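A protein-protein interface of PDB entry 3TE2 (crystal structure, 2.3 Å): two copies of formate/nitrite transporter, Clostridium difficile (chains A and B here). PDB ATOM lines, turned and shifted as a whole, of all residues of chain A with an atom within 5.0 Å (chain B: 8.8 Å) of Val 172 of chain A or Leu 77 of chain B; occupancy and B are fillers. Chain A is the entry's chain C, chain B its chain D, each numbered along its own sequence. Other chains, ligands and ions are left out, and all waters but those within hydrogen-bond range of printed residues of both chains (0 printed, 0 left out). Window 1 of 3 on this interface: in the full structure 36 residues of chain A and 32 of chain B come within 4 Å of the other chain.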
ATOM      1  N   ASN A 167     -20.498 -27.581 -41.401  1.00  0.00           N
ATOM      2  CA  ASN A 167     -21.495 -28.600 -41.082  1.00  0.00           C
ATOM      3  C   ASN A 167     -21.655 -28.839 -39.586  1.00  0.00           C
ATOM      4  O   ASN A 167     -22.691 -29.332 -39.135  1.00  0.00           O
ATOM      5  CB  ASN A 167     -21.231 -29.910 -41.828  1.00  0.00           C
ATOM      6  CG  ASN A 167     -22.515 -30.647 -42.158  1.00  0.00           C
ATOM      7  OD1 ASN A 167     -23.602 -30.071 -42.101  1.00  0.00           O
ATOM      8  ND2 ASN A 167     -22.399 -31.923 -42.505  1.00  0.00           N
ATOM      9  N   ILE A 168     -20.630 -28.487 -38.818  1.00  0.00           N
ATOM     10  CA  ILE A 168     -20.779 -28.411 -37.373  1.00  0.00           C
ATOM     11  C   ILE A 168     -21.881 -27.407 -37.066  1.00  0.00           C
ATOM     12  O   ILE A 168     -22.769 -27.664 -36.254  1.00  0.00           O
ATOM     13  CB  ILE A 168     -19.475 -27.974 -36.685  1.00  0.00           C
ATOM     14  CG1 ILE A 168     -18.523 -29.166 -36.563  1.00  0.00           C
ATOM     15  CG2 ILE A 168     -19.770 -27.383 -35.311  1.00  0.00           C
ATOM     16  CD1 ILE A 168     -17.197 -28.842 -35.905  1.00  0.00           C
ATOM     17  N   LEU A 169     -21.831 -26.270 -37.749  1.00  0.00           N
ATOM     18  CA  LEU A 169     -22.805 -25.207 -37.543  1.00  0.00           C
ATOM     19  C   LEU A 169     -24.174 -25.532 -38.141  1.00  0.00           C
ATOM     20  O   LEU A 169     -25.204 -25.267 -37.518  1.00  0.00           O
ATOM     21  CB  LEU A 169     -22.271 -23.874 -38.076  1.00  0.00           C
ATOM     22  CG  LEU A 169     -21.444 -23.098 -37.046  1.00  0.00           C
ATOM     23  CD1 LEU A 169     -20.585 -22.034 -37.709  1.00  0.00           C
ATOM     24  CD2 LEU A 169     -22.363 -22.490 -35.984  1.00  0.00           C
ATOM     25  N   VAL A 170     -24.193 -26.112 -39.338  1.00  0.00           N
ATOM     26  CA  VAL A 170     -25.465 -26.522 -39.923  1.00  0.00           C
ATOM     27  C   VAL A 170     -26.117 -27.620 -39.087  1.00  0.00           C
ATOM     28  O   VAL A 170     -27.312 -27.557 -38.793  1.00  0.00           O
ATOM     29  CB  VAL A 170     -25.322 -26.993 -41.380  1.00  0.00           C
ATOM     30  CG1 VAL A 170     -26.516 -27.852 -41.773  1.00  0.00           C
ATOM     31  CG2 VAL A 170     -25.193 -25.798 -42.316  1.00  0.00           C
ATOM     32  N   CYS A 171     -25.333 -28.619 -38.691  1.00  0.00           N
ATOM     33  CA  CYS A 171     -25.888 -29.736 -37.939  1.00  0.00           C
ATOM     34  C   CYS A 171     -26.276 -29.380 -36.506  1.00  0.00           C
ATOM     35  O   CYS A 171     -27.287 -29.869 -36.002  1.00  0.00           O
ATOM     36  CB  CYS A 171     -24.957 -30.950 -37.970  1.00  0.00           C
ATOM     37  SG  CYS A 171     -25.105 -31.926 -39.482  1.00  0.00           S
ATOM     38  N   VAL A 172     -25.492 -28.534 -35.844  1.00  0.00           N
ATOM     39  CA  VAL A 172     -25.852 -28.159 -34.483  1.00  0.00           C
ATOM     40  C   VAL A 172     -27.169 -27.381 -34.481  1.00  0.00           C
ATOM     41  O   VAL A 172     -27.936 -27.433 -33.516  1.00  0.00           O
ATOM     42  CB  VAL A 172     -24.751 -27.364 -33.764  1.00  0.00           C
ATOM     43  CG1 VAL A 172     -24.790 -25.895 -34.170  1.00  0.00           C
ATOM     44  CG2 VAL A 172     -24.912 -27.507 -32.258  1.00  0.00           C
ATOM     45  N   SER A 173     -27.443 -26.677 -35.573  1.00  0.00           N
ATOM     46  CA  SER A 173     -28.710 -25.969 -35.693  1.00  0.00           C
ATOM     47  C   SER A 173     -29.850 -26.971 -35.900  1.00  0.00           C
ATOM     48  O   SER A 173     -30.946 -26.795 -35.369  1.00  0.00           O
ATOM     49  CB  SER A 173     -28.659 -24.924 -36.815  1.00  0.00           C
ATOM     50  OG  SER A 173     -28.901 -25.504 -38.085  1.00  0.00           O
ATOM     51  N   VAL A 174     -29.580 -28.030 -36.660  1.00  0.00           N
ATOM     52  CA  VAL A 174     -30.529 -29.128 -36.790  1.00  0.00           C
ATOM     53  C   VAL A 174     -30.707 -29.817 -35.437  1.00  0.00           C
ATOM     54  O   VAL A 174     -31.817 -30.221 -35.073  1.00  0.00           O
ATOM     55  CB  VAL A 174     -30.082 -30.159 -37.857  1.00  0.00           C
ATOM     56  CG1 VAL A 174     -30.928 -31.425 -37.773  1.00  0.00           C
ATOM     57  CG2 VAL A 174     -30.162 -29.549 -39.255  1.00  0.00           C
ATOM     58  N   LEU A 175     -29.610 -29.933 -34.693  1.00  0.00           N
ATOM     59  CA  LEU A 175     -29.634 -30.502 -33.347  1.00  0.00           C
ATOM     60  C   LEU A 175     -30.533 -29.697 -32.412  1.00  0.00           C
ATOM     61  O   LEU A 175     -31.285 -30.267 -31.620  1.00  0.00           O
ATOM     62  CB  LEU A 175     -28.216 -30.578 -32.771  1.00  0.00           C
ATOM     63  CG  LEU A 175     -28.078 -31.149 -31.355  1.00  0.00           C
ATOM     64  CD1 LEU A 175     -28.701 -32.539 -31.263  1.00  0.00           C
ATOM     65  CD2 LEU A 175     -26.619 -31.183 -30.930  1.00  0.00           C
ATOM     66  N   CYS A 176     -30.455 -28.373 -32.508  1.00  0.00           N
ATOM     67  CA  CYS A 176     -31.293 -27.500 -31.689  1.00  0.00           C
ATOM     68  C   CYS A 176     -32.774 -27.682 -32.003  1.00  0.00           C
ATOM     69  O   CYS A 176     -33.620 -27.611 -31.113  1.00  0.00           O
ATOM     70  CB  CYS A 176     -30.889 -26.030 -31.856  1.00  0.00           C
ATOM     71  SG  CYS A 176     -29.261 -25.631 -31.153  1.00  0.00           S
ATOM     72  N   MET A 189     -32.192 -20.014 -33.728  1.00  0.00           N
ATOM     73  CA  MET A 189     -30.928 -20.746 -33.652  1.00  0.00           C
ATOM     74  C   MET A 189     -30.356 -20.980 -35.041  1.00  0.00           C
ATOM     75  O   MET A 189     -29.147 -20.940 -35.230  1.00  0.00           O
ATOM     76  CB  MET A 189     -31.083 -22.079 -32.909  1.00  0.00           C
ATOM     77  CG  MET A 189     -31.410 -21.925 -31.434  1.00  0.00           C
ATOM     78  SD  MET A 189     -30.278 -20.771 -30.626  1.00  0.00           S
ATOM     79  CE  MET A 189     -28.722 -21.649 -30.806  1.00  0.00           C
ATOM     80  N   CYS A 193     -26.728 -19.632 -36.432  1.00  0.00           N
ATOM     81  CA  CYS A 193     -25.713 -20.538 -36.949  1.00  0.00           C
ATOM     82  C   CYS A 193     -25.320 -20.226 -38.391  1.00  0.00           C
ATOM     83  O   CYS A 193     -24.159 -20.378 -38.767  1.00  0.00           O
ATOM     84  CB  CYS A 193     -26.170 -21.993 -36.816  1.00  0.00           C
ATOM     85  SG  CYS A 193     -26.304 -22.563 -35.107  1.00  0.00           S
ATOM     86  N   MET A 248     -20.532 -34.075 -34.863  1.00  0.00           N
ATOM     87  CA  MET A 248     -21.885 -33.958 -34.325  1.00  0.00           C
ATOM     88  C   MET A 248     -22.577 -35.309 -34.166  1.00  0.00           C
ATOM     89  O   MET A 248     -23.259 -35.555 -33.169  1.00  0.00           O
ATOM     90  CB  MET A 248     -22.727 -33.018 -35.193  1.00  0.00           C
ATOM     91  CG  MET A 248     -22.149 -31.613 -35.327  1.00  0.00           C
ATOM     92  SD  MET A 248     -21.869 -30.804 -33.737  1.00  0.00           S
ATOM     93  CE  MET A 248     -23.488 -30.951 -32.988  1.00  0.00           C
ATOM     94  N   PHE B  36     -17.657 -29.749 -26.257  1.00  0.00           N
ATOM     95  CA  PHE B  36     -18.677 -29.143 -27.112  1.00  0.00           C
ATOM     96  C   PHE B  36     -18.929 -27.688 -26.722  1.00  0.00           C
ATOM     97  O   PHE B  36     -18.916 -26.797 -27.573  1.00  0.00           O
ATOM     98  CB  PHE B  36     -19.987 -29.933 -27.031  1.00  0.00           C
ATOM     99  CG  PHE B  36     -20.165 -30.938 -28.135  1.00  0.00           C
ATOM    100  CD1 PHE B  36     -19.994 -30.572 -29.459  1.00  0.00           C
ATOM    101  CD2 PHE B  36     -20.505 -32.251 -27.847  1.00  0.00           C
ATOM    102  CE1 PHE B  36     -20.162 -31.494 -30.477  1.00  0.00           C
ATOM    103  CE2 PHE B  36     -20.673 -33.178 -28.859  1.00  0.00           C
ATOM    104  CZ  PHE B  36     -20.501 -32.799 -30.176  1.00  0.00           C
ATOM    105  N   ALA B  37     -19.160 -27.459 -25.431  1.00  0.00           N
ATOM    106  CA  ALA B  37     -19.440 -26.119 -24.919  1.00  0.00           C
ATOM    107  C   ALA B  37     -18.313 -25.144 -25.232  1.00  0.00           C
ATOM    108  O   ALA B  37     -18.554 -24.031 -25.700  1.00  0.00           O
ATOM    109  CB  ALA B  37     -19.702 -26.163 -23.418  1.00  0.00           C
ATOM    110  N   LEU B  39     -16.177 -25.312 -27.597  1.00  0.00           N
ATOM    111  CA  LEU B  39     -16.115 -25.085 -29.034  1.00  0.00           C
ATOM    112  C   LEU B  39     -17.267 -24.189 -29.497  1.00  0.00           C
ATOM    113  O   LEU B  39     -17.079 -23.292 -30.326  1.00  0.00           O
ATOM    114  CB  LEU B  39     -16.117 -26.423 -29.784  1.00  0.00           C
ATOM    115  CG  LEU B  39     -16.044 -26.372 -31.312  1.00  0.00           C
ATOM    116  CD1 LEU B  39     -15.360 -27.618 -31.875  1.00  0.00           C
ATOM    117  CD2 LEU B  39     -17.434 -26.198 -31.903  1.00  0.00           C
ATOM    118  N   TYR B  40     -18.454 -24.434 -28.951  1.00  0.00           N
ATOM    119  CA  TYR B  40     -19.625 -23.616 -29.254  1.00  0.00           C
ATOM    120  C   TYR B  40     -19.361 -22.153 -28.896  1.00  0.00           C
ATOM    121  O   TYR B  40     -19.713 -21.246 -29.652  1.00  0.00           O
ATOM    122  CB  TYR B  40     -20.850 -24.118 -28.486  1.00  0.00           C
ATOM    123  CG  TYR B  40     -21.394 -25.449 -28.950  1.00  0.00           C
ATOM    124  CD1 TYR B  40     -21.193 -25.895 -30.249  1.00  0.00           C
ATOM    125  CD2 TYR B  40     -22.122 -26.258 -28.085  1.00  0.00           C
ATOM    126  CE1 TYR B  40     -21.700 -27.113 -30.673  1.00  0.00           C
ATOM    127  CE2 TYR B  40     -22.629 -27.473 -28.496  1.00  0.00           C
ATOM    128  CZ  TYR B  40     -22.415 -27.897 -29.790  1.00  0.00           C
ATOM    129  OH  TYR B  40     -22.920 -29.113 -30.195  1.00  0.00           O
ATOM    130  N   VAL B  41     -18.750 -21.933 -27.733  1.00  0.00           N
ATOM    131  CA  VAL B  41     -18.372 -20.588 -27.304  1.00  0.00           C
ATOM    132  C   VAL B  41     -17.319 -20.006 -28.240  1.00  0.00           C
ATOM    133  O   VAL B  41     -17.407 -18.845 -28.647  1.00  0.00           O
ATOM    134  CB  VAL B  41     -17.834 -20.573 -25.857  1.00  0.00           C
ATOM    135  CG1 VAL B  41     -17.111 -19.275 -25.571  1.00  0.00           C
ATOM    136  CG2 VAL B  41     -18.967 -20.781 -24.859  1.00  0.00           C
ATOM    137  N   GLY B  42     -16.328 -20.823 -28.586  1.00  0.00           N
ATOM    138  CA  GLY B  42     -15.287 -20.405 -29.507  1.00  0.00           C
ATOM    139  C   GLY B  42     -15.849 -20.004 -30.860  1.00  0.00           C
ATOM    140  O   GLY B  42     -15.278 -19.160 -31.550  1.00  0.00           O
ATOM    141  N   ILE B  43     -16.967 -20.616 -31.247  1.00  0.00           N
ATOM    142  CA  ILE B  43     -17.582 -20.325 -32.538  1.00  0.00           C
ATOM    143  C   ILE B  43     -18.081 -18.884 -32.552  1.00  0.00           C
ATOM    144  O   ILE B  43     -17.955 -18.180 -33.555  1.00  0.00           O
ATOM    145  CB  ILE B  43     -18.722 -21.324 -32.868  1.00  0.00           C
ATOM    146  CG1 ILE B  43     -18.143 -22.562 -33.558  1.00  0.00           C
ATOM    147  CG2 ILE B  43     -19.786 -20.678 -33.754  1.00  0.00           C
ATOM    148  CD1 ILE B  43     -19.146 -23.666 -33.776  1.00  0.00           C
ATOM    149  N   GLY B  44     -18.630 -18.442 -31.425  1.00  0.00           N
ATOM    150  CA  GLY B  44     -18.976 -17.042 -31.260  1.00  0.00           C
ATOM    151  C   GLY B  44     -17.775 -16.140 -31.488  1.00  0.00           C
ATOM    152  O   GLY B  44     -17.888 -15.091 -32.121  1.00  0.00           O
ATOM    153  N   PHE B  71     -22.667 -11.843 -30.680  1.00  0.00           N
ATOM    154  CA  PHE B  71     -22.031 -12.869 -29.855  1.00  0.00           C
ATOM    155  C   PHE B  71     -23.032 -13.861 -29.250  1.00  0.00           C
ATOM    156  O   PHE B  71     -22.635 -14.891 -28.706  1.00  0.00           O
ATOM    157  CB  PHE B  71     -21.172 -12.211 -28.758  1.00  0.00           C
ATOM    158  CG  PHE B  71     -20.244 -13.171 -28.044  1.00  0.00           C
ATOM    159  CD1 PHE B  71     -19.297 -13.904 -28.750  1.00  0.00           C
ATOM    160  CD2 PHE B  71     -20.308 -13.326 -26.669  1.00  0.00           C
ATOM    161  CE1 PHE B  71     -18.440 -14.782 -28.097  1.00  0.00           C
ATOM    162  CE2 PHE B  71     -19.448 -14.196 -26.009  1.00  0.00           C
ATOM    163  CZ  PHE B  71     -18.512 -14.924 -26.725  1.00  0.00           C
ATOM    164  N   ALA B  72     -24.324 -13.559 -29.368  1.00  0.00           N
ATOM    165  CA  ALA B  72     -25.381 -14.386 -28.771  1.00  0.00           C
ATOM    166  C   ALA B  72     -25.243 -15.892 -29.027  1.00  0.00           C
ATOM    167  O   ALA B  72     -25.521 -16.710 -28.146  1.00  0.00           O
ATOM    168  CB  ALA B  72     -26.745 -13.904 -29.226  1.00  0.00           C
ATOM    169  N   ILE B  73     -24.821 -16.261 -30.232  1.00  0.00           N
ATOM    170  CA  ILE B  73     -24.696 -17.676 -30.576  1.00  0.00           C
ATOM    171  C   ILE B  73     -23.890 -18.476 -29.540  1.00  0.00           C
ATOM    172  O   ILE B  73     -24.215 -19.624 -29.242  1.00  0.00           O
ATOM    173  CB  ILE B  73     -24.058 -17.854 -31.963  1.00  0.00           C
ATOM    174  CG1 ILE B  73     -24.077 -19.329 -32.377  1.00  0.00           C
ATOM    175  CG2 ILE B  73     -22.636 -17.290 -31.971  1.00  0.00           C
ATOM    176  CD1 ILE B  73     -23.644 -19.556 -33.820  1.00  0.00           C
ATOM    177  N   ALA B  74     -22.843 -17.865 -28.992  1.00  0.00           N
ATOM    178  CA  ALA B  74     -21.954 -18.554 -28.060  1.00  0.00           C
ATOM    179  C   ALA B  74     -22.698 -19.263 -26.920  1.00  0.00           C
ATOM    180  O   ALA B  74     -22.648 -20.489 -26.796  1.00  0.00           O
ATOM    181  CB  ALA B  74     -20.908 -17.587 -27.507  1.00  0.00           C
ATOM    182  N   LEU B  75     -23.389 -18.496 -26.086  1.00  0.00           N
ATOM    183  CA  LEU B  75     -24.112 -19.082 -24.961  1.00  0.00           C
ATOM    184  C   LEU B  75     -25.456 -19.694 -25.380  1.00  0.00           C
ATOM    185  O   LEU B  75     -25.959 -20.611 -24.726  1.00  0.00           O
ATOM    186  CB  LEU B  75     -24.301 -18.048 -23.846  1.00  0.00           C
ATOM    187  CG  LEU B  75     -24.737 -18.595 -22.485  1.00  0.00           C
ATOM    188  CD1 LEU B  75     -23.879 -19.789 -22.058  1.00  0.00           C
ATOM    189  CD2 LEU B  75     -24.694 -17.498 -21.435  1.00  0.00           C
ATOM    190  N   SER B  76     -26.040 -19.185 -26.465  1.00  0.00           N
ATOM    191  CA  SER B  76     -27.273 -19.766 -26.996  1.00  0.00           C
ATOM    192  C   SER B  76     -27.083 -21.246 -27.344  1.00  0.00           C
ATOM    193  O   SER B  76     -27.943 -22.076 -27.050  1.00  0.00           O
ATOM    194  CB  SER B  76     -27.765 -18.991 -28.222  1.00  0.00           C
ATOM    195  OG  SER B  76     -27.975 -17.623 -27.909  1.00  0.00           O
ATOM    196  N   LEU B  77     -25.955 -21.574 -27.969  1.00  0.00           N
ATOM    197  CA  LEU B  77     -25.669 -22.961 -28.341  1.00  0.00           C
ATOM    198  C   LEU B  77     -25.478 -23.832 -27.109  1.00  0.00           C
ATOM    199  O   LEU B  77     -26.016 -24.933 -27.025  1.00  0.00           O
ATOM    200  CB  LEU B  77     -24.425 -23.049 -29.227  1.00  0.00           C
ATOM    201  CG  LEU B  77     -24.602 -22.682 -30.697  1.00  0.00           C
ATOM    202  CD1 LEU B  77     -23.266 -22.752 -31.434  1.00  0.00           C
ATOM    203  CD2 LEU B  77     -25.632 -23.597 -31.340  1.00  0.00           C
ATOM    204  N   VAL B  78     -24.703 -23.327 -26.157  1.00  0.00           N
ATOM    205  CA  VAL B  78     -24.469 -24.028 -24.905  1.00  0.00           C
ATOM    206  C   VAL B  78     -25.796 -24.402 -24.240  1.00  0.00           C
ATOM    207  O   VAL B  78     -26.042 -25.570 -23.926  1.00  0.00           O
ATOM    208  CB  VAL B  78     -23.614 -23.171 -23.944  1.00  0.00           C
ATOM    209  CG1 VAL B  78     -23.694 -23.711 -22.517  1.00  0.00           C
ATOM    210  CG2 VAL B  78     -22.168 -23.105 -24.433  1.00  0.00           C
ATOM    211  N   ILE B  79     -26.650 -23.405 -24.039  1.00  0.00           N
ATOM    212  CA  ILE B  79     -27.929 -23.605 -23.367  1.00  0.00           C
ATOM    213  C   ILE B  79     -28.867 -24.526 -24.144  1.00  0.00           C
ATOM    214  O   ILE B  79     -29.491 -25.420 -23.564  1.00  0.00           O
ATOM    215  CB  ILE B  79     -28.640 -22.258 -23.110  1.00  0.00           C
ATOM    216  CG1 ILE B  79     -27.864 -21.440 -22.075  1.00  0.00           C
ATOM    217  CG2 ILE B  79     -30.070 -22.485 -22.646  1.00  0.00           C
ATOM    218  CD1 ILE B  79     -27.691 -22.156 -20.760  1.00  0.00           C
ATOM    219  N   MET B  80     -28.967 -24.308 -25.452  1.00  0.00           N
ATOM    220  CA  MET B  80     -29.873 -25.100 -26.286  1.00  0.00           C
ATOM    221  C   MET B  80     -29.406 -26.549 -26.489  1.00  0.00           C
ATOM    222  O   MET B  80     -30.211 -27.419 -26.820  1.00  0.00           O
ATOM    223  CB  MET B  80     -30.125 -24.409 -27.633  1.00  0.00           C
ATOM    224  CG  MET B  80     -30.915 -23.113 -27.522  1.00  0.00           C
ATOM    225  SD  MET B  80     -32.557 -23.320 -26.793  1.00  0.00           S
ATOM    226  CE  MET B  80     -33.491 -23.924 -28.197  1.00  0.00           C
ATOM    227  N   THR B  81     -28.117 -26.808 -26.282  1.00  0.00           N
ATOM    228  CA  THR B  81     -27.589 -28.169 -26.412  1.00  0.00           C
ATOM    229  C   THR B  81     -27.433 -28.876 -25.060  1.00  0.00           C
ATOM    230  O   THR B  81     -27.175 -30.079 -25.005  1.00  0.00           O
ATOM    231  CB  THR B  81     -26.229 -28.196 -27.153  1.00  0.00           C
ATOM    232  OG1 THR B  81     -25.273 -27.395 -26.443  1.00  0.00           O
ATOM    233  CG2 THR B  81     -26.378 -27.673 -28.571  1.00  0.00           C
ATOM    234  N   GLY B  82     -27.588 -28.130 -23.974  1.00  0.00           N
ATOM    235  CA  GLY B  82     -27.429 -28.694 -22.643  1.00  0.00           C
ATOM    236  C   GLY B  82     -26.031 -29.224 -22.360  1.00  0.00           C
ATOM    237  O   GLY B  82     -25.874 -30.252 -21.700  1.00  0.00           O
ATOM    238  N   THR B  83     -25.012 -28.526 -22.855  1.00  0.00           N
ATOM    239  CA  THR B  83     -23.623 -28.933 -22.632  1.00  0.00           C
ATOM    240  C   THR B  83     -22.989 -28.205 -21.438  1.00  0.00           C
ATOM    241  O   THR B  83     -23.509 -27.194 -20.968  1.00  0.00           O
ATOM    242  CB  THR B  83     -22.764 -28.742 -23.899  1.00  0.00           C
ATOM    243  OG1 THR B  83     -23.063 -27.475 -24.495  1.00  0.00           O
ATOM    244  CG2 THR B  83     -23.057 -29.844 -24.915  1.00  0.00           C
ATOM    245  N   GLU B  84     -21.867 -28.731 -20.951  1.00  0.00           N
ATOM    246  CA  GLU B  84     -21.247 -28.248 -19.719  1.00  0.00           C
ATOM    247  C   GLU B  84     -20.276 -27.097 -19.960  1.00  0.00           C
ATOM    248  O   GLU B  84     -19.267 -27.266 -20.639  1.00  0.00           O
ATOM    249  CB  GLU B  84     -20.512 -29.393 -19.008  1.00  0.00           C
ATOM    250  CG  GLU B  84     -21.413 -30.499 -18.475  1.00  0.00           C
ATOM    251  CD  GLU B  84     -22.162 -30.098 -17.215  1.00  0.00           C
ATOM    252  OE1 GLU B  84     -21.550 -29.474 -16.319  1.00  0.00           O
ATOM    253  OE2 GLU B  84     -23.367 -30.405 -17.122  1.00  0.00           O
ATOM    254  N   LEU B  85     -20.586 -25.934 -19.387  1.00  0.00           N
ATOM    255  CA  LEU B  85     -19.736 -24.754 -19.499  1.00  0.00           C
ATOM    256  C   LEU B  85     -19.198 -24.365 -18.133  1.00  0.00           C
ATOM    257  O   LEU B  85     -19.965 -24.169 -17.184  1.00  0.00           O
ATOM    258  CB  LEU B  85     -20.515 -23.570 -20.086  1.00  0.00           C
ATOM    259  CG  LEU B  85     -19.705 -22.290 -20.317  1.00  0.00           C
ATOM    260  CD1 LEU B  85     -18.579 -22.551 -21.305  1.00  0.00           C
ATOM    261  CD2 LEU B  85     -20.589 -21.135 -20.799  1.00  0.00           C
ATOM    262  N   ILE B 187     -33.166 -17.368 -25.113  1.00  0.00           N
ATOM    263  CA  ILE B 187     -32.239 -16.864 -26.115  1.00  0.00           C
ATOM    264  C   ILE B 187     -32.187 -15.333 -26.159  1.00  0.00           C
ATOM    265  O   ILE B 187     -31.116 -14.757 -26.332  1.00  0.00           O
ATOM    266  CB  ILE B 187     -32.560 -17.428 -27.516  1.00  0.00           C
ATOM    267  CG1 ILE B 187     -32.376 -18.948 -27.516  1.00  0.00           C
ATOM    268  CG2 ILE B 187     -31.669 -16.771 -28.572  1.00  0.00           C
ATOM    269  CD1 ILE B 187     -33.118 -19.674 -28.631  1.00  0.00           C
ATOM    270  N   ILE B 190     -30.088 -14.162 -23.307  1.00  0.00           N
ATOM    271  CA  ILE B 190     -28.696 -14.516 -23.536  1.00  0.00           C
ATOM    272  C   ILE B 190     -28.099 -13.488 -24.479  1.00  0.00           C
ATOM    273  O   ILE B 190     -27.011 -12.955 -24.240  1.00  0.00           O
ATOM    274  CB  ILE B 190     -28.565 -15.929 -24.139  1.00  0.00           C
ATOM    275  CG1 ILE B 190     -28.918 -16.987 -23.090  1.00  0.00           C
ATOM    276  CG2 ILE B 190     -27.162 -16.146 -24.689  1.00  0.00           C
ATOM    277  CD1 ILE B 190     -28.987 -18.417 -23.629  1.00  0.00           C
ATOM    278  N   LEU B 194     -24.975 -11.093 -23.316  1.00  0.00           N
ATOM    279  CA  LEU B 194     -23.725 -11.201 -24.061  1.00  0.00           C
ATOM    280  C   LEU B 194     -23.431  -9.902 -24.821  1.00  0.00           C
ATOM    281  O   LEU B 194     -22.275  -9.505 -24.956  1.00  0.00           O
ATOM    282  CB  LEU B 194     -23.738 -12.428 -24.990  1.00  0.00           C
ATOM    283  CG  LEU B 194     -23.128 -13.712 -24.384  1.00  0.00           C
ATOM    284  CD1 LEU B 194     -23.762 -14.073 -23.037  1.00  0.00           C
ATOM    285  CD2 LEU B 194     -23.208 -14.890 -25.342  1.00  0.00           C
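SG of Cys 193 of chain A sits close to O of Leu 169 of chain A (3.8 Å). The backbone carbonyl oxygen (O) of Val 172 of chain A lies within hydrogen-bond range of the side-chain sulfur (SG) of Cys 176 of chain A (3.3 Å). The backbone carbonyl oxygen (O) of Met 189 of chain A is in hydrogen-bond range of the side-chain sulfur (SG) of Cys 193 of chain A, at 3.3 Å. O of Ala 72 of chain B is in hydrogen-bond range of OG of Ser 76 of chain B. The side-chain hydroxyl (OG1) of Thr 81 of chain B lies within hydrogen-bond range of the backbone carbonyl oxygen (O) of Leu 77 of chain B (2.6 Å). The backbone carbonyl oxygen (O) of Val 78 of chain B lies within hydrogen-bond range of the side-chain hydroxyl (OG1) of Thr 81 of chain B (3.2 Å).
Among the printed residues, merely in contact across the chains: Val 172 of chain A with Tyr 40 of chain B (3.3 Å), Met 248 of chain A with Tyr 40 of chain B (3.4 Å), Met 189 of chain A with Ile 187 of chain B (3.6 Å), Met 189 of chain A with Leu 77 of chain B (3.7 Å), Val 172 of chain A with Leu 77 of chain B (3.7 Å), Met 248 of chain A with Phe 36 of chain B (3.7 Å), Cys 176 of chain A with Met 80 of chain B (3.8 Å), Met 189 of chain A with Ser 76 of chain B (3.8 Å), Leu 169 of chain A with Ile 43 of chain B (3.9 Å), Leu 169 of chain A with Ile 73 of chain B (3.9 Å), Cys 193 of chain A with Ile 73 of chain B (3.9 Å), Met 189 of chain A with Met 80 of chain B (3.9 Å), Cys 193 of chain A with Leu 77 of chain B (3.96 Å) and Val 172 of chain A with Thr 81 of chain B (3.97 Å).
Cys 171 of chain A touches none of the printed residues of chain B. Val 172 of chain A touches just these residues of chain B: Tyr 40, Leu 77 and Thr 81. No residue of chain B comes within 4 Å of Ser 173 of chain A. Val 174 of chain A touches none of the printed residues of chain B. Of the printed residues of chain B, Cys 176 of chain A touches Met 80 (3.8 Å). Printed residues of chain A within 4 Å of Phe 36 of chain B: Met 248. Printed residues of chain A within 4 Å of Tyr 40 of chain B: Val 172 and Met 248. Of chain A, only Val 172 (3.7 Å), Met 189 (3.7 Å) and Cys 193 (3.96 Å) come within 4 Å of Leu 77 of chain B. Of the printed residues of chain A, Thr 81 of chain B touches Val 172 (3.97 Å). Of the printed residues of chain A, Ile 187 of chain B touches Met 189. The nearest residue of chain A that does not touch Leu 77 of chain B is Cys 176 of chain A (4.2 Å). The nearest printed residue of chain A that does not touch Ile 187 of chain B is Cys 176 of chain A (7.5 Å).
Of the 26 printed residues of chain B, 9 touch a printed residue of chain A. Hydrophobic or aromatic side chains of chain B that line the printed part of chain A: Phe 36, Tyr 40, Ile 43, Ile 73, Leu 77, Met 80 and Ile 187. Of the 13 printed residues of chain A, 6 touch a printed residue of chain B.
No position is printed for both chains. Of the 14 pairs that touch across the chains among the printed residues, none has its exchanged pair printed and touching as well.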
